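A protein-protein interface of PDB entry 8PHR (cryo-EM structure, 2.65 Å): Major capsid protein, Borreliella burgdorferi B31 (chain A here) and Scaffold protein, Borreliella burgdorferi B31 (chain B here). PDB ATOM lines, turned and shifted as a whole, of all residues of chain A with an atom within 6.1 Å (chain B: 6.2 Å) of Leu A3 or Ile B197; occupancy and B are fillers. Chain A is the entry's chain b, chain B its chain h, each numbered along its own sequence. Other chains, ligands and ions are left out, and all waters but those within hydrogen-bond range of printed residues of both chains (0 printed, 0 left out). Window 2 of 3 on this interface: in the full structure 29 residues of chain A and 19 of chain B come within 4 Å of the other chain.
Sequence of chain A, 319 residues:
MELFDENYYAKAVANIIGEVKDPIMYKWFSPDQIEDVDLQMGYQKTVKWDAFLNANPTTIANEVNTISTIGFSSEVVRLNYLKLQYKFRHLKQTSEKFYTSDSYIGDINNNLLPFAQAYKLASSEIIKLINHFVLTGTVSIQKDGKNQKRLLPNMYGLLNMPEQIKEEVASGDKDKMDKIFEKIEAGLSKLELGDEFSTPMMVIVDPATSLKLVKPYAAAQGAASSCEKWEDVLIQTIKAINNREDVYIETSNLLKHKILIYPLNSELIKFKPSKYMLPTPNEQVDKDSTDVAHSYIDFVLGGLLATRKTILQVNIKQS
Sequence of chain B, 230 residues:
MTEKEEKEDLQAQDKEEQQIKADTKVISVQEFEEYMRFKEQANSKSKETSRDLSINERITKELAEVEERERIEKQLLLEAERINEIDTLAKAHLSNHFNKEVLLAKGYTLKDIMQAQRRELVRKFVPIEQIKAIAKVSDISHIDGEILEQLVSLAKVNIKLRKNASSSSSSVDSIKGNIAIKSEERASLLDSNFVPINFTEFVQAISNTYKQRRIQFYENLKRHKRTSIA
The side-chain amide oxygen (OD1) of Asn B198 is in hydrogen-bond range of the backbone NH (N) of Glu B201. The backbone NH of Ile B197 is in hydrogen-bond range of the side-chain carboxylate of Glu B201 (3.1 Å).
Among the printed residues, pairs that only touch across the chains: Leu A3 with Pro B196 (3.4 Å), Leu A3 with Ile B197 (3.5 Å), Leu A3 with Asn B198 (3.4 Å), Leu A3 with Phe B202 (3.8 Å), Phe A4 with Pro B196 (3.5 Å), Ala A10 with Phe B202 (3.4 Å) and Glu A283 with Phe B199 (3.3 Å).
Ile B197 touches just one residue of chain A: Leu A3 (3.5 Å). Of the printed residues of chain B, Phe A4 touches Pro B196 (3.5 Å). Of the printed residues of chain A, Phe B199 touches Glu A283 (3.3 Å). Printed residues of chain A within 4 Å of Phe B202: Leu A3 (3.8 Å) and Ala A10 (3.4 Å). Of the printed residues of chain A, Asn B198 touches Leu A3 (3.4 Å). Glu B201 touches none of the printed residues of chain A. Asp A5 touches none of the printed residues of chain B. The nearest residue of chain B that does not touch Leu A3 is Phe B199 (4.02 Å). The nearest residue of chain A that does not touch Ile B197 is Glu A6 (5.9 Å). The nearest printed residue of chain A that does not touch Asn B198 is Glu A283 (6.6 Å).
Of the 8 printed residues of chain B, 5 touch a printed residue of chain A. Along chain B the printed residues that touch a printed residue of chain A span positions 196 to 202. Of the 8 printed residues of chain A, 4 touch a printed residue of chain B. Hydrophobic or aromatic side chains of chain A within 4 Å of the printed part of chain B: Leu A3 and Phe A4.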
ATOM      1  N   LEU A   3      -2.709   7.749 -22.674  1.00  0.00           N
ATOM      2  CA  LEU A   3      -2.932   6.309 -22.744  1.00  0.00           C
ATOM      3  C   LEU A   3      -2.536   5.631 -21.437  1.00  0.00           C
ATOM      4  O   LEU A   3      -3.238   4.744 -20.950  1.00  0.00           O
ATOM      5  CB  LEU A   3      -2.152   5.702 -23.913  1.00  0.00           C
ATOM      6  CG  LEU A   3      -1.878   4.198 -23.840  1.00  0.00           C
ATOM      7  CD1 LEU A   3      -3.130   3.408 -24.189  1.00  0.00           C
ATOM      8  CD2 LEU A   3      -0.726   3.815 -24.754  1.00  0.00           C
ATOM      9  N   PHE A   4      -1.401   6.056 -20.874  1.00  0.00           N
ATOM     10  CA  PHE A   4      -0.941   5.483 -19.614  1.00  0.00           C
ATOM     11  C   PHE A   4      -1.890   5.807 -18.468  1.00  0.00           C
ATOM     12  O   PHE A   4      -2.062   4.988 -17.558  1.00  0.00           O
ATOM     13  CB  PHE A   4       0.468   5.982 -19.290  1.00  0.00           C
ATOM     14  CG  PHE A   4       1.550   5.322 -20.098  1.00  0.00           C
ATOM     15  CD1 PHE A   4       1.275   4.208 -20.875  1.00  0.00           C
ATOM     16  CD2 PHE A   4       2.845   5.813 -20.077  1.00  0.00           C
ATOM     17  CE1 PHE A   4       2.270   3.599 -21.617  1.00  0.00           C
ATOM     18  CE2 PHE A   4       3.845   5.208 -20.816  1.00  0.00           C
ATOM     19  CZ  PHE A   4       3.557   4.100 -21.587  1.00  0.00           C
ATOM     20  N   ASP A   5      -2.505   6.992 -18.487  1.00  0.00           N
ATOM     21  CA  ASP A   5      -3.466   7.342 -17.447  1.00  0.00           C
ATOM     22  C   ASP A   5      -4.686   6.430 -17.493  1.00  0.00           C
ATOM     23  O   ASP A   5      -5.181   5.987 -16.450  1.00  0.00           O
ATOM     24  CB  ASP A   5      -3.888   8.804 -17.591  1.00  0.00           C
ATOM     25  CG  ASP A   5      -2.708   9.752 -17.607  1.00  0.00           C
ATOM     26  OD1 ASP A   5      -1.558   9.273 -17.513  1.00  0.00           O
ATOM     27  OD2 ASP A   5      -2.929  10.975 -17.716  1.00  0.00           O
ATOM     28  N   GLU A   6      -5.181   6.136 -18.697  1.00  0.00           N
ATOM     29  CA  GLU A   6      -6.361   5.290 -18.833  1.00  0.00           C
ATOM     30  C   GLU A   6      -6.038   3.832 -18.529  1.00  0.00           C
ATOM     31  O   GLU A   6      -6.796   3.154 -17.827  1.00  0.00           O
ATOM     32  CB  GLU A   6      -6.945   5.428 -20.241  1.00  0.00           C
ATOM     33  CG  GLU A   6      -7.438   6.825 -20.583  1.00  0.00           C
ATOM     34  CD  GLU A   6      -7.915   6.938 -22.019  1.00  0.00           C
ATOM     35  OE1 GLU A   6      -7.762   5.957 -22.776  1.00  0.00           O
ATOM     36  OE2 GLU A   6      -8.441   8.009 -22.392  1.00  0.00           O
ATOM     37  N   ASN A   7      -4.919   3.333 -19.050  1.00  0.00           N
ATOM     38  CA  ASN A   7      -4.534   1.932 -18.921  1.00  0.00           C
ATOM     39  C   ASN A   7      -3.274   1.839 -18.067  1.00  0.00           C
ATOM     40  O   ASN A   7      -2.208   2.315 -18.471  1.00  0.00           O
ATOM     41  CB  ASN A   7      -4.313   1.307 -20.296  1.00  0.00           C
ATOM     42  CG  ASN A   7      -4.284  -0.206 -20.253  1.00  0.00           C
ATOM     43  OD1 ASN A   7      -4.435  -0.813 -19.192  1.00  0.00           O
ATOM     44  ND2 ASN A   7      -4.090  -0.827 -21.410  1.00  0.00           N
ATOM     45  N   TYR A   8      -3.399   1.226 -16.886  1.00  0.00           N
ATOM     46  CA  TYR A   8      -2.229   1.013 -16.040  1.00  0.00           C
ATOM     47  C   TYR A   8      -1.345  -0.109 -16.571  1.00  0.00           C
ATOM     48  O   TYR A   8      -0.122  -0.068 -16.393  1.00  0.00           O
ATOM     49  CB  TYR A   8      -2.657   0.706 -14.606  1.00  0.00           C
ATOM     50  CG  TYR A   8      -1.497   0.447 -13.668  1.00  0.00           C
ATOM     51  CD1 TYR A   8      -0.727   1.493 -13.180  1.00  0.00           C
ATOM     52  CD2 TYR A   8      -1.163  -0.846 -13.285  1.00  0.00           C
ATOM     53  CE1 TYR A   8       0.336   1.262 -12.325  1.00  0.00           C
ATOM     54  CE2 TYR A   8      -0.103  -1.088 -12.431  1.00  0.00           C
ATOM     55  CZ  TYR A   8       0.644  -0.031 -11.955  1.00  0.00           C
ATOM     56  OH  TYR A   8       1.701  -0.266 -11.106  1.00  0.00           O
ATOM     57  N   ALA A  10      -0.508  -0.887 -19.613  1.00  0.00           N
ATOM     58  CA  ALA A  10       0.453  -0.369 -20.581  1.00  0.00           C
ATOM     59  C   ALA A  10       1.614   0.328 -19.883  1.00  0.00           C
ATOM     60  O   ALA A  10       2.775   0.166 -20.276  1.00  0.00           O
ATOM     61  CB  ALA A  10      -0.241   0.580 -21.556  1.00  0.00           C
ATOM     62  N   GLU A 283      -4.030  -5.615 -26.113  1.00  0.00           N
ATOM     63  CA  GLU A 283      -4.905  -4.667 -25.430  1.00  0.00           C
ATOM     64  C   GLU A 283      -6.026  -5.373 -24.677  1.00  0.00           C
ATOM     65  O   GLU A 283      -6.531  -4.842 -23.682  1.00  0.00           O
ATOM     66  CB  GLU A 283      -5.487  -3.673 -26.436  1.00  0.00           C
ATOM     67  CG  GLU A 283      -6.084  -2.426 -25.806  1.00  0.00           C
ATOM     68  CD  GLU A 283      -6.546  -1.416 -26.837  1.00  0.00           C
ATOM     69  OE1 GLU A 283      -6.428  -1.703 -28.047  1.00  0.00           O
ATOM     70  OE2 GLU A 283      -7.029  -0.335 -26.439  1.00  0.00           O
ATOM     71  N   PHE B 194       8.551  10.744 -24.392  1.00  0.00           N
ATOM     72  CA  PHE B 194       7.565  10.095 -25.247  1.00  0.00           C
ATOM     73  C   PHE B 194       6.313   9.763 -24.445  1.00  0.00           C
ATOM     74  O   PHE B 194       6.378   9.034 -23.450  1.00  0.00           O
ATOM     75  CB  PHE B 194       8.153   8.830 -25.865  1.00  0.00           C
ATOM     76  CG  PHE B 194       7.123   7.920 -26.465  1.00  0.00           C
ATOM     77  CD1 PHE B 194       6.371   8.325 -27.555  1.00  0.00           C
ATOM     78  CD2 PHE B 194       6.894   6.664 -25.929  1.00  0.00           C
ATOM     79  CE1 PHE B 194       5.418   7.490 -28.106  1.00  0.00           C
ATOM     80  CE2 PHE B 194       5.942   5.827 -26.473  1.00  0.00           C
ATOM     81  CZ  PHE B 194       5.204   6.239 -27.564  1.00  0.00           C
ATOM     82  N   VAL B 195       5.178  10.298 -24.876  1.00  0.00           N
ATOM     83  CA  VAL B 195       3.886  10.034 -24.260  1.00  0.00           C
ATOM     84  C   VAL B 195       2.988   9.379 -25.302  1.00  0.00           C
ATOM     85  O   VAL B 195       2.450  10.050 -26.183  1.00  0.00           O
ATOM     86  CB  VAL B 195       3.248  11.323 -23.710  1.00  0.00           C
ATOM     87  CG1 VAL B 195       1.874  11.026 -23.126  1.00  0.00           C
ATOM     88  CG2 VAL B 195       4.153  11.957 -22.668  1.00  0.00           C
ATOM     89  N   PRO B 196       2.817   8.058 -25.242  1.00  0.00           N
ATOM     90  CA  PRO B 196       1.955   7.384 -26.222  1.00  0.00           C
ATOM     91  C   PRO B 196       0.511   7.847 -26.104  1.00  0.00           C
ATOM     92  O   PRO B 196       0.012   8.136 -25.014  1.00  0.00           O
ATOM     93  CB  PRO B 196       2.100   5.900 -25.865  1.00  0.00           C
ATOM     94  CG  PRO B 196       2.557   5.889 -24.445  1.00  0.00           C
ATOM     95  CD  PRO B 196       3.384   7.123 -24.257  1.00  0.00           C
ATOM     96  N   ILE B 197      -0.163   7.913 -27.251  1.00  0.00           N
ATOM     97  CA  ILE B 197      -1.545   8.373 -27.303  1.00  0.00           C
ATOM     98  C   ILE B 197      -2.483   7.172 -27.314  1.00  0.00           C
ATOM     99  O   ILE B 197      -3.578   7.223 -26.743  1.00  0.00           O
ATOM    100  CB  ILE B 197      -1.787   9.275 -28.527  1.00  0.00           C
ATOM    101  CG1 ILE B 197      -0.795  10.439 -28.537  1.00  0.00           C
ATOM    102  CG2 ILE B 197      -3.218   9.797 -28.535  1.00  0.00           C
ATOM    103  CD1 ILE B 197      -0.964  11.382 -29.711  1.00  0.00           C
ATOM    104  N   ASN B 198      -2.059   6.082 -27.949  1.00  0.00           N
ATOM    105  CA  ASN B 198      -2.916   4.914 -28.084  1.00  0.00           C
ATOM    106  C   ASN B 198      -2.066   3.650 -28.114  1.00  0.00           C
ATOM    107  O   ASN B 198      -0.832   3.696 -28.159  1.00  0.00           O
ATOM    108  CB  ASN B 198      -3.796   5.013 -29.336  1.00  0.00           C
ATOM    109  CG  ASN B 198      -3.002   5.356 -30.581  1.00  0.00           C
ATOM    110  OD1 ASN B 198      -2.216   4.546 -31.072  1.00  0.00           O
ATOM    111  ND2 ASN B 198      -3.201   6.563 -31.097  1.00  0.00           N
ATOM    112  N   PHE B 199      -2.758   2.507 -28.091  1.00  0.00           N
ATOM    113  CA  PHE B 199      -2.075   1.221 -28.026  1.00  0.00           C
ATOM    114  C   PHE B 199      -1.274   0.939 -29.290  1.00  0.00           C
ATOM    115  O   PHE B 199      -0.243   0.261 -29.225  1.00  0.00           O
ATOM    116  CB  PHE B 199      -3.085   0.101 -27.776  1.00  0.00           C
ATOM    117  CG  PHE B 199      -2.506  -1.084 -27.060  1.00  0.00           C
ATOM    118  CD1 PHE B 199      -2.136  -0.990 -25.730  1.00  0.00           C
ATOM    119  CD2 PHE B 199      -2.327  -2.289 -27.716  1.00  0.00           C
ATOM    120  CE1 PHE B 199      -1.601  -2.075 -25.064  1.00  0.00           C
ATOM    121  CE2 PHE B 199      -1.792  -3.380 -27.056  1.00  0.00           C
ATOM    122  CZ  PHE B 199      -1.429  -3.271 -25.729  1.00  0.00           C
ATOM    123  N   GLU B 201       0.387   3.220 -31.106  1.00  0.00           N
ATOM    124  CA  GLU B 201       1.642   3.935 -30.897  1.00  0.00           C
ATOM    125  C   GLU B 201       2.492   3.247 -29.841  1.00  0.00           C
ATOM    126  O   GLU B 201       3.723   3.207 -29.954  1.00  0.00           O
ATOM    127  CB  GLU B 201       1.369   5.388 -30.504  1.00  0.00           C
ATOM    128  CG  GLU B 201       0.482   6.151 -31.474  1.00  0.00           C
ATOM    129  CD  GLU B 201       0.311   7.606 -31.084  1.00  0.00           C
ATOM    130  OE1 GLU B 201       0.949   8.038 -30.101  1.00  0.00           O
ATOM    131  OE2 GLU B 201      -0.461   8.319 -31.758  1.00  0.00           O
ATOM    132  N   PHE B 202       1.855   2.697 -28.804  1.00  0.00           N
ATOM    133  CA  PHE B 202       2.604   1.978 -27.777  1.00  0.00           C
ATOM    134  C   PHE B 202       3.309   0.754 -28.357  1.00  0.00           C
ATOM    135  O   PHE B 202       4.474   0.489 -28.041  1.00  0.00           O
ATOM    136  CB  PHE B 202       1.664   1.580 -26.638  1.00  0.00           C
ATOM    137  CG  PHE B 202       2.335   0.829 -25.527  1.00  0.00           C
ATOM    138  CD1 PHE B 202       3.407   1.384 -24.848  1.00  0.00           C
ATOM    139  CD2 PHE B 202       1.884  -0.424 -25.147  1.00  0.00           C
ATOM    140  CE1 PHE B 202       4.025   0.699 -23.819  1.00  0.00           C
ATOM    141  CE2 PHE B 202       2.496  -1.113 -24.117  1.00  0.00           C
ATOM    142  CZ  PHE B 202       3.568  -0.551 -23.454  1.00  0.00           C
